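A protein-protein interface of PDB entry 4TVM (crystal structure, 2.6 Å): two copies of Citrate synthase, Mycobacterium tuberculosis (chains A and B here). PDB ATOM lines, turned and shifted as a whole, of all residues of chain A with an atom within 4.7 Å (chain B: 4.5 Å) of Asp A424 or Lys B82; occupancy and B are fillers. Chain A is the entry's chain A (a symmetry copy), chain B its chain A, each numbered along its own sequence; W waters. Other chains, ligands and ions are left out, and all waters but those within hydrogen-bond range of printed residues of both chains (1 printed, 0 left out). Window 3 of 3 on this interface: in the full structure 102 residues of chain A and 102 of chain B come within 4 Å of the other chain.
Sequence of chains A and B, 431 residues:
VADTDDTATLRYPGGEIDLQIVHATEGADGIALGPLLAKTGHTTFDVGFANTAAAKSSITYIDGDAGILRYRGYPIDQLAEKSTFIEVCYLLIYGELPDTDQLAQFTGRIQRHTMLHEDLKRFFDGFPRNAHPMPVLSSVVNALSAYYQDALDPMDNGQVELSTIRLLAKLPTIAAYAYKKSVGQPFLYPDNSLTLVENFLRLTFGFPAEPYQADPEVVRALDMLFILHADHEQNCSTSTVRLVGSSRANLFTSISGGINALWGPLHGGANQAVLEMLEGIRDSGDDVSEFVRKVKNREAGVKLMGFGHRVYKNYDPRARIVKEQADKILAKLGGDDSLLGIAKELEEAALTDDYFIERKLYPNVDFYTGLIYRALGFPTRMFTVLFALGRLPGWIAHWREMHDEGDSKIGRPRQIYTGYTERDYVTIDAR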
ATOM      1  N   GLU A 422      12.865  32.215   8.365  1.00  0.00           N
ATOM      2  CA  GLU A 422      13.198  31.537   7.017  1.00  0.00           C
ATOM      3  C   GLU A 422      12.809  30.019   6.695  1.00  0.00           C
ATOM      4  O   GLU A 422      12.395  29.276   7.566  1.00  0.00           O
ATOM      5  CB  GLU A 422      14.755  31.675   6.818  1.00  0.00           C
ATOM      6  CG  GLU A 422      15.634  31.378   8.078  1.00  0.00           C
ATOM      7  CD  GLU A 422      17.136  31.712   7.941  1.00  0.00           C
ATOM      8  OE1 GLU A 422      17.553  32.164   6.867  1.00  0.00           O
ATOM      9  OE2 GLU A 422      17.934  31.537   8.908  1.00  0.00           O
ATOM     10  N   ARG A 423      13.020  29.548   5.455  1.00  0.00           N
ATOM     11  CA  ARG A 423      12.692  28.146   5.043  1.00  0.00           C
ATOM     12  C   ARG A 423      13.868  27.238   4.622  1.00  0.00           C
ATOM     13  O   ARG A 423      14.727  27.670   3.885  1.00  0.00           O
ATOM     14  CB  ARG A 423      11.785  28.182   3.823  1.00  0.00           C
ATOM     15  CG  ARG A 423      10.326  27.890   4.067  1.00  0.00           C
ATOM     16  CD  ARG A 423       9.582  28.526   2.924  1.00  0.00           C
ATOM     17  NE  ARG A 423       9.236  29.919   3.215  1.00  0.00           N
ATOM     18  CZ  ARG A 423       9.637  31.007   2.533  1.00  0.00           C
ATOM     19  NH1 ARG A 423      10.417  30.944   1.444  1.00  0.00           N
ATOM     20  NH2 ARG A 423       9.231  32.197   2.942  1.00  0.00           N
ATOM     21  N   ASP A 424      13.859  25.975   5.050  1.00  0.00           N
ATOM     22  CA  ASP A 424      14.949  25.007   4.807  1.00  0.00           C
ATOM     23  C   ASP A 424      15.246  24.858   3.319  1.00  0.00           C
ATOM     24  O   ASP A 424      14.356  24.633   2.521  1.00  0.00           O
ATOM     25  CB  ASP A 424      14.618  23.611   5.413  1.00  0.00           C
ATOM     26  CG  ASP A 424      15.849  22.619   5.445  1.00  0.00           C
ATOM     27  OD1 ASP A 424      16.721  22.750   6.327  1.00  0.00           O
ATOM     28  OD2 ASP A 424      15.932  21.648   4.635  1.00  0.00           O
ATOM     29  N   TYR A 425      16.511  24.967   2.962  1.00  0.00           N
ATOM     30  CA  TYR A 425      16.916  24.612   1.634  1.00  0.00           C
ATOM     31  C   TYR A 425      17.946  23.525   1.754  1.00  0.00           C
ATOM     32  O   TYR A 425      18.794  23.562   2.646  1.00  0.00           O
ATOM     33  CB  TYR A 425      17.421  25.814   0.852  1.00  0.00           C
ATOM     34  CG  TYR A 425      18.346  26.727   1.591  1.00  0.00           C
ATOM     35  CD1 TYR A 425      17.854  27.690   2.467  1.00  0.00           C
ATOM     36  CD2 TYR A 425      19.715  26.668   1.376  1.00  0.00           C
ATOM     37  CE1 TYR A 425      18.711  28.559   3.128  1.00  0.00           C
ATOM     38  CE2 TYR A 425      20.581  27.526   2.029  1.00  0.00           C
ATOM     39  CZ  TYR A 425      20.079  28.467   2.905  1.00  0.00           C
ATOM     40  OH  TYR A 425      20.950  29.308   3.552  1.00  0.00           O
ATOM     41  N   VAL A 426      17.813  22.522   0.891  1.00  0.00           N
ATOM     42  CA  VAL A 426      18.656  21.352   0.930  1.00  0.00           C
ATOM     43  C   VAL A 426      20.086  21.827   0.713  1.00  0.00           C
ATOM     44  O   VAL A 426      20.314  22.882   0.073  1.00  0.00           O
ATOM     45  CB  VAL A 426      18.153  20.274  -0.082  1.00  0.00           C
ATOM     46  CG1 VAL A 426      19.221  19.808  -1.056  1.00  0.00           C
ATOM     47  CG2 VAL A 426      17.566  19.080   0.652  1.00  0.00           C
ATOM     48  N   TYR B  74      13.970  28.864  11.186  1.00  0.00           N
ATOM     49  CA  TYR B  74      13.512  27.660  10.506  1.00  0.00           C
ATOM     50  C   TYR B  74      12.540  26.870  11.361  1.00  0.00           C
ATOM     51  O   TYR B  74      12.841  26.581  12.502  1.00  0.00           O
ATOM     52  CB  TYR B  74      14.683  26.768  10.192  1.00  0.00           C
ATOM     53  CG  TYR B  74      15.702  27.385   9.282  1.00  0.00           C
ATOM     54  CD1 TYR B  74      15.420  27.583   7.927  1.00  0.00           C
ATOM     55  CD2 TYR B  74      16.961  27.754   9.754  1.00  0.00           C
ATOM     56  CE1 TYR B  74      16.351  28.147   7.076  1.00  0.00           C
ATOM     57  CE2 TYR B  74      17.904  28.307   8.907  1.00  0.00           C
ATOM     58  CZ  TYR B  74      17.598  28.495   7.574  1.00  0.00           C
ATOM     59  OH  TYR B  74      18.526  29.026   6.721  1.00  0.00           O
ATOM     60  N   GLN B  78      10.136  21.331   9.822  1.00  0.00           N
ATOM     61  CA  GLN B  78      11.054  21.196   8.676  1.00  0.00           C
ATOM     62  C   GLN B  78      12.416  20.572   9.067  1.00  0.00           C
ATOM     63  O   GLN B  78      12.924  19.680   8.382  1.00  0.00           O
ATOM     64  CB  GLN B  78      11.231  22.559   7.962  1.00  0.00           C
ATOM     65  CG  GLN B  78      10.093  22.923   7.000  1.00  0.00           C
ATOM     66  CD  GLN B  78      10.144  24.356   6.457  1.00  0.00           C
ATOM     67  OE1 GLN B  78       9.169  25.116   6.523  1.00  0.00           O
ATOM     68  NE2 GLN B  78      11.257  24.719   5.899  1.00  0.00           N
ATOM     69  N   LEU B  79      12.993  20.982  10.194  1.00  0.00           N
ATOM     70  CA  LEU B  79      14.307  20.421  10.617  1.00  0.00           C
ATOM     71  C   LEU B  79      14.174  18.988  11.052  1.00  0.00           C
ATOM     72  O   LEU B  79      15.022  18.137  10.749  1.00  0.00           O
ATOM     73  CB  LEU B  79      14.885  21.236  11.762  1.00  0.00           C
ATOM     74  CG  LEU B  79      14.965  22.729  11.488  1.00  0.00           C
ATOM     75  CD1 LEU B  79      14.972  23.489  12.797  1.00  0.00           C
ATOM     76  CD2 LEU B  79      16.166  23.041  10.612  1.00  0.00           C
ATOM     77  N   ALA B  80      13.095  18.715  11.777  1.00  0.00           N
ATOM     78  CA  ALA B  80      12.829  17.376  12.290  1.00  0.00           C
ATOM     79  C   ALA B  80      12.741  16.410  11.139  1.00  0.00           C
ATOM     80  O   ALA B  80      13.402  15.378  11.122  1.00  0.00           O
ATOM     81  CB  ALA B  80      11.530  17.363  13.081  1.00  0.00           C
ATOM     82  N   GLU B  81      11.905  16.767  10.174  1.00  0.00           N
ATOM     83  CA  GLU B  81      11.688  15.952   8.994  1.00  0.00           C
ATOM     84  C   GLU B  81      12.851  16.002   8.000  1.00  0.00           C
ATOM     85  O   GLU B  81      13.154  14.971   7.384  1.00  0.00           O
ATOM     86  CB  GLU B  81      10.351  16.334   8.340  1.00  0.00           C
ATOM     87  CG  GLU B  81       9.155  16.091   9.274  1.00  0.00           C
ATOM     88  CD  GLU B  81       9.003  14.623   9.678  1.00  0.00           C
ATOM     89  OE1 GLU B  81       9.379  13.749   8.863  1.00  0.00           O
ATOM     90  OE2 GLU B  81       8.516  14.338  10.801  1.00  0.00           O
ATOM     91  N   LYS B  82      13.528  17.146   7.858  1.00  0.00           N
ATOM     92  CA  LYS B  82      14.603  17.252   6.831  1.00  0.00           C
ATOM     93  C   LYS B  82      16.087  17.433   7.252  1.00  0.00           C
ATOM     94  O   LYS B  82      16.983  17.310   6.405  1.00  0.00           O
ATOM     95  CB  LYS B  82      14.242  18.348   5.825  1.00  0.00           C
ATOM     96  CG  LYS B  82      13.236  17.889   4.788  1.00  0.00           C
ATOM     97  CD  LYS B  82      13.828  16.746   3.965  1.00  0.00           C
ATOM     98  CE  LYS B  82      12.818  16.160   2.999  1.00  0.00           C
ATOM     99  NZ  LYS B  82      12.164  17.212   2.174  1.00  0.00           N
ATOM    100  N   SER B  83      16.362  17.709   8.525  1.00  0.00           N
ATOM    101  CA  SER B  83      17.735  17.963   8.957  1.00  0.00           C
ATOM    102  C   SER B  83      18.344  16.782   9.696  1.00  0.00           C
ATOM    103  O   SER B  83      17.833  15.667   9.637  1.00  0.00           O
ATOM    104  CB  SER B  83      17.800  19.212   9.840  1.00  0.00           C
ATOM    105  OG  SER B  83      19.141  19.604  10.016  1.00  0.00           O
ATOM    106  N   LEU B  97      22.508  27.575   8.422  1.00  0.00           N
ATOM    107  CA  LEU B  97      22.753  26.217   7.924  1.00  0.00           C
ATOM    108  C   LEU B  97      24.107  26.236   7.214  1.00  0.00           C
ATOM    109  O   LEU B  97      24.488  27.275   6.638  1.00  0.00           O
ATOM    110  CB  LEU B  97      21.675  25.747   6.970  1.00  0.00           C
ATOM    111  CG  LEU B  97      20.201  25.756   7.421  1.00  0.00           C
ATOM    112  CD1 LEU B  97      19.251  25.955   6.244  1.00  0.00           C
ATOM    113  CD2 LEU B  97      19.826  24.479   8.155  1.00  0.00           C
HETATM  114  O   HOH W   1      21.017  29.588   6.746  1.00  0.00           O
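Water W1 lies within hydrogen-bond range of OH of Tyr B74 (2.6 Å), N of Leu B97 (3.0 Å) and OH of Tyr A425 (3.2 Å).
The side-chain amide nitrogen (NE2) of Gln B78 lies close to the backbone NH (N) of Asp A424 (3.0 Å).
OH of Tyr B74 sits close to OE1 of Glu A422.
Printed residues of chain B within 4 Å of Glu A422: Tyr B74 (3.2 Å).
Printed residues of chain B within 4 Å of Arg A423: Tyr B74 (3.6 Å) and Gln B78 (3.8 Å).
Printed residues of chain B within 4 Å of Asp A424: Tyr B74 (3.6 Å), Gln B78 (3.0 Å), Lys B82 (3.9 Å) and Leu B97 (3.997 Å).
Of the printed residues of chain B, Tyr A425 touches Tyr B74.
Val A426 touches none of the printed residues of chain B.
Printed residues of chain A within 4 Å of Tyr B74: Glu A422 (3.2 Å), Arg A423 (3.6 Å), Asp A424 (3.6 Å) and Tyr A425 (3.6 Å).
Of the printed residues of chain A, Gln B78 touches Arg A423 and Asp A424.
Of chain A, only Asp A424 comes within 4 Å of Lys B82.
Ser B83 touches none of the printed residues of chain A.
The nearest printed residue of chain A that does not touch Lys B82 is Val A426 (5.5 Å).
No position is printed for both chains.
Of the 8 pairs that touch across the chains among the printed residues, none has its exchanged pair printed and touching as well.
Printed residues of chain A that touch a printed residue of chain B: Glu A422, Arg A423, Asp A424 and Tyr A425.
Hydrophobic or aromatic side chains of chain A within 4 Å of the printed part of chain B: Tyr A425.
Of the 8 printed residues of chain B, 4 touch a printed residue of chain A.
C of Arg A423 touches CE1 of Tyr B74 (3.6 Å).
Arg A423 touches Gln B78 (CG to NE2, 3.8 Å).
Asp A424 touches Tyr B74 (N to CD1, 3.6 Å).
Lys B82 touches Asp A424 (CB to OD2, 3.9 Å).
CD2 of Leu B97 touches OD1 of Asp A424, at 3.997 Å.
Tyr B74 touches Tyr A425 (OH to CE1, 3.6 Å).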
